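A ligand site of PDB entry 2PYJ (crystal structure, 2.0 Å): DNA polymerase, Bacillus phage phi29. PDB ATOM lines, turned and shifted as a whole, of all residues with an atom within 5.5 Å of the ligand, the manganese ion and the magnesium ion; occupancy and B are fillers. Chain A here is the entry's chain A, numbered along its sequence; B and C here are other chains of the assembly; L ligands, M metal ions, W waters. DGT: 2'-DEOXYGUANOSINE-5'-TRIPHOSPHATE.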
ATOM      1  N   ASP A 249      27.400  27.134  23.094  1.00  0.00           N
ATOM      2  CA  ASP A 249      26.262  26.218  23.331  1.00  0.00           C
ATOM      3  C   ASP A 249      26.696  24.804  22.981  1.00  0.00           C
ATOM      4  O   ASP A 249      27.187  24.561  21.889  1.00  0.00           O
ATOM      5  CB  ASP A 249      25.066  26.627  22.429  1.00  0.00           C
ATOM      6  CG  ASP A 249      23.764  25.852  22.759  1.00  0.00           C
ATOM      7  OD1 ASP A 249      22.856  26.512  23.315  1.00  0.00           O
ATOM      8  OD2 ASP A 249      23.631  24.611  22.460  1.00  0.00           O
ATOM      9  N   VAL A 250      26.508  23.867  23.913  1.00  0.00           N
ATOM     10  CA  VAL A 250      26.910  22.482  23.652  1.00  0.00           C
ATOM     11  C   VAL A 250      26.083  21.874  22.501  1.00  0.00           C
ATOM     12  O   VAL A 250      24.823  22.034  22.425  1.00  0.00           O
ATOM     13  CB  VAL A 250      26.827  21.576  24.907  1.00  0.00           C
ATOM     14  CG1 VAL A 250      27.246  20.125  24.543  1.00  0.00           C
ATOM     15  CG2 VAL A 250      27.724  22.097  25.999  1.00  0.00           C
ATOM     16  N   ASN A 251      26.805  21.218  21.581  1.00  0.00           N
ATOM     17  CA  ASN A 251      26.192  20.411  20.537  1.00  0.00           C
ATOM     18  C   ASN A 251      25.577  19.156  21.146  1.00  0.00           C
ATOM     19  O   ASN A 251      26.291  18.302  21.655  1.00  0.00           O
ATOM     20  CB  ASN A 251      27.208  20.060  19.459  1.00  0.00           C
ATOM     21  CG  ASN A 251      27.861  21.282  18.843  1.00  0.00           C
ATOM     22  OD1 ASN A 251      27.210  22.317  18.634  1.00  0.00           O
ATOM     23  ND2 ASN A 251      29.161  21.186  18.562  1.00  0.00           N
ATOM     24  N   SER A 252      24.244  19.079  21.136  1.00  0.00           N
ATOM     25  CA  SER A 252      23.493  17.935  21.699  1.00  0.00           C
ATOM     26  C   SER A 252      23.932  17.548  23.113  1.00  0.00           C
ATOM     27  O   SER A 252      24.476  16.454  23.308  1.00  0.00           O
ATOM     28  CB  SER A 252      23.610  16.701  20.778  1.00  0.00           C
ATOM     29  OG  SER A 252      22.959  16.914  19.540  1.00  0.00           O
ATOM     30  N   LEU A 253      23.692  18.428  24.094  1.00  0.00           N
ATOM     31  CA  LEU A 253      24.221  18.215  25.451  1.00  0.00           C
ATOM     32  C   LEU A 253      23.740  16.937  26.139  1.00  0.00           C
ATOM     33  O   LEU A 253      24.539  16.160  26.626  1.00  0.00           O
ATOM     34  CB  LEU A 253      23.992  19.415  26.392  1.00  0.00           C
ATOM     35  CG  LEU A 253      24.595  19.198  27.805  1.00  0.00           C
ATOM     36  CD1 LEU A 253      26.132  19.069  27.790  1.00  0.00           C
ATOM     37  CD2 LEU A 253      24.170  20.271  28.818  1.00  0.00           C
ATOM     38  N   TYR A 254      22.431  16.724  26.197  1.00  0.00           N
ATOM     39  CA  TYR A 254      21.910  15.556  26.916  1.00  0.00           C
ATOM     40  C   TYR A 254      22.338  14.237  26.227  1.00  0.00           C
ATOM     41  O   TYR A 254      22.768  13.319  26.904  1.00  0.00           O
ATOM     42  CB  TYR A 254      20.390  15.625  27.103  1.00  0.00           C
ATOM     43  CG  TYR A 254      19.883  16.642  28.131  1.00  0.00           C
ATOM     44  CD1 TYR A 254      18.644  16.469  28.730  1.00  0.00           C
ATOM     45  CD2 TYR A 254      20.644  17.771  28.479  1.00  0.00           C
ATOM     46  CE1 TYR A 254      18.144  17.398  29.663  1.00  0.00           C
ATOM     47  CE2 TYR A 254      20.154  18.710  29.412  1.00  0.00           C
ATOM     48  CZ  TYR A 254      18.892  18.512  29.988  1.00  0.00           C
ATOM     49  OH  TYR A 254      18.399  19.412  30.915  1.00  0.00           O
ATOM     50  N   PRO A 255      22.199  14.140  24.879  1.00  0.00           N
ATOM     51  CA  PRO A 255      22.737  12.981  24.150  1.00  0.00           C
ATOM     52  C   PRO A 255      24.260  12.762  24.324  1.00  0.00           C
ATOM     53  O   PRO A 255      24.705  11.632  24.285  1.00  0.00           O
ATOM     54  CB  PRO A 255      22.420  13.306  22.678  1.00  0.00           C
ATOM     55  CG  PRO A 255      21.257  14.228  22.743  1.00  0.00           C
ATOM     56  CD  PRO A 255      21.472  15.060  23.965  1.00  0.00           C
ATOM     57  N   LYS A 371      22.119  14.382  12.022  1.00  0.00           N
ATOM     58  CA  LYS A 371      22.145  15.774  12.514  1.00  0.00           C
ATOM     59  C   LYS A 371      23.315  16.609  11.948  1.00  0.00           C
ATOM     60  O   LYS A 371      23.123  17.766  11.551  1.00  0.00           O
ATOM     61  CB  LYS A 371      22.180  15.789  14.048  1.00  0.00           C
ATOM     62  CG  LYS A 371      22.044  17.175  14.670  1.00  0.00           C
ATOM     63  CD  LYS A 371      21.846  17.064  16.165  1.00  0.00           C
ATOM     64  CE  LYS A 371      21.893  18.413  16.852  1.00  0.00           C
ATOM     65  NZ  LYS A 371      23.257  18.784  17.295  1.00  0.00           N
ATOM     66  N   LYS A 383      17.883  15.926  15.740  1.00  0.00           N
ATOM     67  CA  LYS A 383      18.016  16.491  17.085  1.00  0.00           C
ATOM     68  C   LYS A 383      16.879  16.023  18.015  1.00  0.00           C
ATOM     69  O   LYS A 383      17.120  15.644  19.167  1.00  0.00           O
ATOM     70  CB  LYS A 383      18.046  18.025  17.012  1.00  0.00           C
ATOM     71  CG  LYS A 383      17.940  18.753  18.356  1.00  0.00           C
ATOM     72  CD  LYS A 383      18.188  20.226  18.170  1.00  0.00           C
ATOM     73  CE  LYS A 383      17.828  21.025  19.398  1.00  0.00           C
ATOM     74  NZ  LYS A 383      18.399  22.413  19.311  1.00  0.00           N
ATOM     75  N   LEU A 384      15.648  16.040  17.487  1.00  0.00           N
ATOM     76  CA  LEU A 384      14.490  15.601  18.240  1.00  0.00           C
ATOM     77  C   LEU A 384      14.518  14.088  18.536  1.00  0.00           C
ATOM     78  O   LEU A 384      14.099  13.685  19.620  1.00  0.00           O
ATOM     79  CB  LEU A 384      13.193  15.995  17.494  1.00  0.00           C
ATOM     80  CG  LEU A 384      11.832  15.645  18.121  1.00  0.00           C
ATOM     81  CD1 LEU A 384      11.686  16.183  19.527  1.00  0.00           C
ATOM     82  CD2 LEU A 384      10.692  16.141  17.220  1.00  0.00           C
ATOM     83  N   ASN A 387      16.896  13.872  21.525  1.00  0.00           N
ATOM     84  CA  ASN A 387      16.360  14.463  22.749  1.00  0.00           C
ATOM     85  C   ASN A 387      15.100  13.782  23.295  1.00  0.00           C
ATOM     86  O   ASN A 387      14.905  13.705  24.512  1.00  0.00           O
ATOM     87  CB  ASN A 387      16.117  15.969  22.555  1.00  0.00           C
ATOM     88  CG  ASN A 387      17.412  16.745  22.408  1.00  0.00           C
ATOM     89  OD1 ASN A 387      18.467  16.316  22.878  1.00  0.00           O
ATOM     90  ND2 ASN A 387      17.344  17.902  21.761  1.00  0.00           N
ATOM     91  N   SER A 388      14.247  13.278  22.397  1.00  0.00           N
ATOM     92  CA  SER A 388      12.999  12.618  22.803  1.00  0.00           C
ATOM     93  C   SER A 388      13.236  11.226  23.372  1.00  0.00           C
ATOM     94  O   SER A 388      12.414  10.719  24.116  1.00  0.00           O
ATOM     95  CB  SER A 388      11.974  12.573  21.665  1.00  0.00           C
ATOM     96  OG  SER A 388      12.382  11.732  20.610  1.00  0.00           O
ATOM     97  N   TYR A 390      15.764  10.589  25.482  1.00  0.00           N
ATOM     98  CA  TYR A 390      15.929  11.003  26.871  1.00  0.00           C
ATOM     99  C   TYR A 390      14.550  11.188  27.526  1.00  0.00           C
ATOM    100  O   TYR A 390      14.256  10.597  28.581  1.00  0.00           O
ATOM    101  CB  TYR A 390      16.767  12.295  26.987  1.00  0.00           C
ATOM    102  CG  TYR A 390      16.277  13.216  28.090  1.00  0.00           C
ATOM    103  CD1 TYR A 390      16.298  12.806  29.432  1.00  0.00           C
ATOM    104  CD2 TYR A 390      15.779  14.485  27.800  1.00  0.00           C
ATOM    105  CE1 TYR A 390      15.853  13.620  30.424  1.00  0.00           C
ATOM    106  CE2 TYR A 390      15.318  15.326  28.817  1.00  0.00           C
ATOM    107  CZ  TYR A 390      15.354  14.880  30.122  1.00  0.00           C
ATOM    108  OH  TYR A 390      14.889  15.694  31.125  1.00  0.00           O
ATOM    109  N   GLY A 391      13.703  11.992  26.894  1.00  0.00           N
ATOM    110  CA  GLY A 391      12.374  12.297  27.414  1.00  0.00           C
ATOM    111  C   GLY A 391      11.546  11.066  27.673  1.00  0.00           C
ATOM    112  O   GLY A 391      10.855  10.980  28.702  1.00  0.00           O
ATOM    113  N   ASP A 456      21.661  28.883  30.198  1.00  0.00           N
ATOM    114  CA  ASP A 456      20.393  28.144  30.096  1.00  0.00           C
ATOM    115  C   ASP A 456      20.635  26.728  29.605  1.00  0.00           C
ATOM    116  O   ASP A 456      20.717  26.488  28.403  1.00  0.00           O
ATOM    117  CB  ASP A 456      19.351  28.862  29.217  1.00  0.00           C
ATOM    118  CG  ASP A 456      17.948  28.237  29.364  1.00  0.00           C
ATOM    119  OD1 ASP A 456      17.832  27.120  29.927  1.00  0.00           O
ATOM    120  OD2 ASP A 456      16.969  28.871  28.914  1.00  0.00           O
ATOM    121  N   THR A 457      20.764  25.821  30.564  1.00  0.00           N
ATOM    122  CA  THR A 457      20.810  24.372  30.322  1.00  0.00           C
ATOM    123  C   THR A 457      22.166  23.881  29.811  1.00  0.00           C
ATOM    124  O   THR A 457      22.775  23.010  30.414  1.00  0.00           O
ATOM    125  CB  THR A 457      19.646  23.888  29.403  1.00  0.00           C
ATOM    126  OG1 THR A 457      18.390  24.334  29.953  1.00  0.00           O
ATOM    127  CG2 THR A 457      19.635  22.374  29.276  1.00  0.00           C
ATOM    128  N   ASP A 458      22.614  24.449  28.692  1.00  0.00           N
ATOM    129  CA  ASP A 458      23.819  23.978  28.009  1.00  0.00           C
ATOM    130  C   ASP A 458      24.572  25.121  27.324  1.00  0.00           C
ATOM    131  O   ASP A 458      25.294  24.899  26.364  1.00  0.00           O
ATOM    132  CB  ASP A 458      23.476  22.860  26.991  1.00  0.00           C
ATOM    133  CG  ASP A 458      22.846  23.393  25.713  1.00  0.00           C
ATOM    134  OD1 ASP A 458      23.047  22.793  24.598  1.00  0.00           O
ATOM    135  OD2 ASP A 458      22.146  24.423  25.810  1.00  0.00           O
ATOM    136  N   SER A 459      24.385  26.339  27.820  1.00  0.00           N
ATOM    137  CA  SER A 459      25.035  27.493  27.244  1.00  0.00           C
ATOM    138  C   SER A 459      25.760  28.287  28.309  1.00  0.00           C
ATOM    139  O   SER A 459      25.384  28.253  29.481  1.00  0.00           O
ATOM    140  CB  SER A 459      24.009  28.396  26.536  1.00  0.00           C
ATOM    141  OG  SER A 459      23.121  28.984  27.464  1.00  0.00           O
ATOM    142  N   GLU A 486      28.271  30.040  19.405  1.00  0.00           N
ATOM    143  CA  GLU A 486      26.953  30.359  18.881  1.00  0.00           C
ATOM    144  C   GLU A 486      26.898  31.768  18.305  1.00  0.00           C
ATOM    145  O   GLU A 486      26.358  31.979  17.213  1.00  0.00           O
ATOM    146  CB  GLU A 486      25.888  30.196  19.959  1.00  0.00           C
ATOM    147  CG  GLU A 486      24.491  30.600  19.514  1.00  0.00           C
ATOM    148  CD  GLU A 486      23.505  30.625  20.649  1.00  0.00           C
ATOM    149  OE1 GLU A 486      23.199  29.538  21.187  1.00  0.00           O
ATOM    150  OE2 GLU A 486      23.039  31.735  21.011  1.00  0.00           O
ATOM    151  P    DC B   4       4.693  10.957  22.635  1.00  0.00           P
ATOM    152  OP1  DC B   4       4.959  12.265  22.004  1.00  0.00           O
ATOM    153  OP2  DC B   4       4.932   9.713  21.898  1.00  0.00           O
ATOM    154  O5'  DC B   4       5.437  10.781  24.026  1.00  0.00           O
ATOM    155  C5'  DC B   4       5.577  11.822  24.942  1.00  0.00           C
ATOM    156  C4'  DC B   4       6.974  11.715  25.496  1.00  0.00           C
ATOM    157  O4'  DC B   4       7.938  11.887  24.415  1.00  0.00           O
ATOM    158  C3'  DC B   4       7.283  12.773  26.527  1.00  0.00           C
ATOM    159  O3'  DC B   4       6.883  12.295  27.820  1.00  0.00           O
ATOM    160  C2'  DC B   4       8.789  12.881  26.380  1.00  0.00           C
ATOM    161  C1'  DC B   4       9.032  12.643  24.886  1.00  0.00           C
ATOM    162  N1   DC B   4       9.187  13.943  24.117  1.00  0.00           N
ATOM    163  C2   DC B   4      10.329  14.728  24.377  1.00  0.00           C
ATOM    164  O2   DC B   4      11.161  14.352  25.202  1.00  0.00           O
ATOM    165  N3   DC B   4      10.481  15.888  23.717  1.00  0.00           N
ATOM    166  C4   DC B   4       9.588  16.299  22.840  1.00  0.00           C
ATOM    167  N4   DC B   4       9.826  17.461  22.247  1.00  0.00           N
ATOM    168  C5   DC B   4       8.415  15.532  22.545  1.00  0.00           C
ATOM    169  C6   DC B   4       8.253  14.372  23.205  1.00  0.00           C
ATOM    170  P    DG B   5       6.383  13.313  28.960  1.00  0.00           P
ATOM    171  OP1  DG B   5       5.955  12.465  30.102  1.00  0.00           O
ATOM    172  OP2  DG B   5       5.499  14.295  28.319  1.00  0.00           O
ATOM    173  O5'  DG B   5       7.699  14.117  29.395  1.00  0.00           O
ATOM    174  C5'  DG B   5       8.759  13.429  30.076  1.00  0.00           C
ATOM    175  C4'  DG B   5       9.913  14.377  30.331  1.00  0.00           C
ATOM    176  O4'  DG B   5      10.510  14.773  29.064  1.00  0.00           O
ATOM    177  C3'  DG B   5       9.512  15.703  30.958  1.00  0.00           C
ATOM    178  O3'  DG B   5       9.342  15.535  32.350  1.00  0.00           O
ATOM    179  C2'  DG B   5      10.727  16.550  30.604  1.00  0.00           C
ATOM    180  C1'  DG B   5      11.078  16.062  29.215  1.00  0.00           C
ATOM    181  N9   DG B   5      10.638  16.946  28.126  1.00  0.00           N
ATOM    182  C8   DG B   5       9.539  16.837  27.297  1.00  0.00           C
ATOM    183  N7   DG B   5       9.452  17.819  26.418  1.00  0.00           N
ATOM    184  C5   DG B   5      10.567  18.622  26.712  1.00  0.00           C
ATOM    185  C6   DG B   5      11.029  19.825  26.124  1.00  0.00           C
ATOM    186  O6   DG B   5      10.509  20.437  25.188  1.00  0.00           O
ATOM    187  N1   DG B   5      12.212  20.320  26.719  1.00  0.00           N
ATOM    188  C2   DG B   5      12.872  19.719  27.771  1.00  0.00           C
ATOM    189  N2   DG B   5      14.002  20.300  28.230  1.00  0.00           N
ATOM    190  N3   DG B   5      12.443  18.588  28.328  1.00  0.00           N
ATOM    191  C4   DG B   5      11.303  18.107  27.754  1.00  0.00           C
ATOM    192  N1  DOC C  10      14.973  24.361  25.782  1.00  0.00           N
ATOM    193  C2  DOC C  10      14.307  23.211  26.269  1.00  0.00           C
ATOM    194  N3  DOC C  10      13.311  22.663  25.533  1.00  0.00           N
ATOM    195  C4  DOC C  10      12.947  23.180  24.339  1.00  0.00           C
ATOM    196  C5  DOC C  10      13.590  24.303  23.839  1.00  0.00           C
ATOM    197  C6  DOC C  10      14.620  24.887  24.589  1.00  0.00           C
ATOM    198  O2  DOC C  10      14.627  22.723  27.368  1.00  0.00           O
ATOM    199  N4  DOC C  10      11.953  22.603  23.649  1.00  0.00           N
ATOM    200  C1' DOC C  10      16.047  24.927  26.618  1.00  0.00           C
ATOM    201  C2' DOC C  10      17.319  24.097  26.430  1.00  0.00           C
ATOM    202  C3' DOC C  10      18.272  25.007  25.696  1.00  0.00           C
ATOM    203  C4' DOC C  10      17.763  26.394  26.004  1.00  0.00           C
ATOM    204  O4' DOC C  10      16.342  26.265  26.234  1.00  0.00           O
ATOM    205  C5' DOC C  10      18.028  27.359  24.849  1.00  0.00           C
ATOM    206  O5' DOC C  10      18.373  28.594  25.461  1.00  0.00           O
ATOM    207  P   DOC C  10      17.693  29.993  25.019  1.00  0.00           P
ATOM    208  OP1 DOC C  10      18.548  31.051  25.634  1.00  0.00           O
ATOM    209  OP2 DOC C  10      17.550  29.972  23.521  1.00  0.00           O
HETATM  210  PG  DGT L   1      22.186  21.766  19.552  1.00  0.00           P
HETATM  211  O1G DGT L   1      21.041  22.178  18.669  1.00  0.00           O
HETATM  212  O2G DGT L   1      23.337  21.215  18.758  1.00  0.00           O
HETATM  213  O3G DGT L   1      22.607  22.700  20.729  1.00  0.00           O
HETATM  214  O3B DGT L   1      21.538  20.482  20.300  1.00  0.00           O
HETATM  215  PB  DGT L   1      21.044  20.419  21.839  1.00  0.00           P
HETATM  216  O1B DGT L   1      20.463  19.032  22.049  1.00  0.00           O
HETATM  217  O2B DGT L   1      22.099  21.044  22.767  1.00  0.00           O
HETATM  218  O3A DGT L   1      19.752  21.400  21.860  1.00  0.00           O
HETATM  219  PA  DGT L   1      19.621  22.719  22.766  1.00  0.00           P
HETATM  220  O1A DGT L   1      18.450  23.500  22.138  1.00  0.00           O
HETATM  221  O2A DGT L   1      21.004  23.396  23.004  1.00  0.00           O
HETATM  222  O5' DGT L   1      19.004  22.131  24.103  1.00  0.00           O
HETATM  223  C5' DGT L   1      19.819  21.706  25.176  1.00  0.00           C
HETATM  224  C4' DGT L   1      19.210  20.494  25.831  1.00  0.00           C
HETATM  225  O4' DGT L   1      17.879  20.767  26.356  1.00  0.00           O
HETATM  226  C3' DGT L   1      19.058  19.280  24.928  1.00  0.00           C
HETATM  227  O3' DGT L   1      20.265  18.528  24.727  1.00  0.00           O
HETATM  228  C2' DGT L   1      18.037  18.490  25.707  1.00  0.00           C
HETATM  229  C1' DGT L   1      17.111  19.591  26.245  1.00  0.00           C
HETATM  230  N9  DGT L   1      16.086  19.744  25.201  1.00  0.00           N
HETATM  231  C8  DGT L   1      16.027  20.661  24.209  1.00  0.00           C
HETATM  232  N7  DGT L   1      14.940  20.412  23.426  1.00  0.00           N
HETATM  233  C5  DGT L   1      14.321  19.338  23.922  1.00  0.00           C
HETATM  234  C6  DGT L   1      13.123  18.538  23.593  1.00  0.00           C
HETATM  235  O6  DGT L   1      12.396  18.827  22.625  1.00  0.00           O
HETATM  236  N1  DGT L   1      12.835  17.486  24.348  1.00  0.00           N
HETATM  237  C2  DGT L   1      13.583  17.119  25.413  1.00  0.00           C
HETATM  238  N2  DGT L   1      13.197  16.034  26.108  1.00  0.00           N
HETATM  239  N3  DGT L   1      14.705  17.808  25.780  1.00  0.00           N
HETATM  240  C4  DGT L   1      15.090  18.894  25.075  1.00  0.00           C
HETATM  241 MN    MN M   1      22.916  22.801  22.657  1.00  0.00          MN
HETATM  242 MG    MG M   2      21.215  25.369  24.090  1.00  0.00          MG
HETATM  243  O   HOH W   1      14.780  18.441  20.277  1.00  0.00           O
HETATM  244  O   HOH W   2      25.265  23.849  19.685  1.00  0.00           O
HETATM  245  O   HOH W   3      21.034  27.087  25.450  1.00  0.00           O
HETATM  246  O   HOH W   4      21.157  21.638  16.086  1.00  0.00           O
HETATM  247  O   HOH W   5      20.397  16.897  20.319  1.00  0.00           O
HETATM  248  O   HOH W   6      14.605  21.956  21.081  1.00  0.00           O
HETATM  249  O   HOH W   7      23.924  22.761  15.783  1.00  0.00           O
HETATM  250  O   HOH W   8      21.393  25.321  20.245  1.00  0.00           O
HETATM  251  O   HOH W   9      19.579  26.270  21.944  1.00  0.00           O
HETATM  252  O   HOH W  10      17.019  25.783  22.229  1.00  0.00           O
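Merely in contact with the magnesium ion: DOC 10 of chain C. Within 4 Å of the magnesium ion: Asp 249, Asp 458 and DOC 10 of chain C. The nearest printed residue that does not touch the magnesium ion is Asp 456 (4.5 Å).
N9 of DG 5 of chain B sits close to a nitrogen (N2) of the ligand (3.4 Å). An oxygen (O1G) of the ligand lies within salt-bridge range of the side-chain amino group (NZ) of Lys 383 (2.7 Å). ND2 of Asn 387 is in hydrogen-bond range of O1B of the ligand, 3.3 Å away. The backbone NH (N) of Leu 253 lies within hydrogen-bond range of an oxygen (O3') of the ligand, at 3.5 Å. The backbone NH (N) of Tyr 254 lies within hydrogen-bond range of an oxygen (O3') of the ligand (3.2 Å). A nitrogen (N2) of the ligand sits at hydrogen-bond distance from the backbone carbonyl oxygen (O) of Asn 387. The side-chain amino group (NZ) of Lys 371 lies within salt-bridge range of an oxygen (O2G) of the ligand (2.8 Å). N2 of the ligand sits at hydrogen-bond distance from O2 of DC 4 of chain B (2.8 Å). The backbone NH (N) of Ser 252 lies within hydrogen-bond range of an oxygen (O3B) of the ligand.
NZ of Lys 371 sits at hydrogen-bond distance from OG of Ser 252 (2.9 Å). The side-chain carboxylate (OD1) of Asp 456 lies within hydrogen-bond range of the side-chain hydroxyl (OG1) of Thr 457, at 2.8 Å. O of Lys 383 lies close to ND2 of Asn 387. N2 of DG 5 of chain B sits close to O2 of DOC 10 of chain C, 2.6 Å away.
A nitrogen (N7) of the ligand sits close to N3 of DOC 10 of chain C, at 3.5 Å. CA of Asn 251 touches O2G of the ligand (3.5 Å). Pro 255 touches the ligand (CD to O3', 3.8 Å). Tyr 390 touches the ligand. CG2 of Thr 457 touches O4' of the ligand, 3.8 Å away. Hydrophobic or aromatic side chains within 4 Å of the ligand: Tyr 254, Pro 255 and Tyr 390. Of the 22 residues printed, 16 come within 4 Å of the ligand.
The manganese ion is bound by an oxygen (O2B) of the ligand (1.9 Å), the side-chain carboxylate (OD1) of Asp 458 (1.9 Å), an oxygen (O3G) of the ligand (2.0 Å), the side-chain carboxylate (OD2) of Asp 249 (2.0 Å), an oxygen (O2A) of the ligand (2.0 Å) and the backbone carbonyl oxygen (O) of Val 250 (2.1 Å).
Water W3 lies within hydrogen-bond range of the backbone carbonyl oxygen (O) of Asp 456 (3.0 Å), O5' of DOC 10 of chain C (3.1 Å) and the side-chain hydroxyl (OG) of Ser 459 (3.5 Å). Water W5 lies within hydrogen-bond range of OG of Ser 252 (2.7 Å), O1B of the ligand (2.7 Å) and OD1 of Asn 387 (3.3 Å). Water W2 lies within hydrogen-bond range of the side-chain amide oxygen (OD1) of Asn 251, the backbone carbonyl oxygen (O) of Asp 249 and an oxygen (O2G) of the ligand. Water W1 bridges the side-chain amide nitrogen of Asn 387 and an oxygen (O6) of the ligand.
The nearest printed residue that does not touch the manganese ion is Ser 252 (4.2 Å).
The magnesium ion is bound by OD1 of Asp 249 (2.1 Å), OD2 of Asp 458 (2.2 Å), water W3 (2.2 Å) and O2A of the ligand (2.3 Å). Slightly farther from the magnesium ion lies water W9 (2.8 Å).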
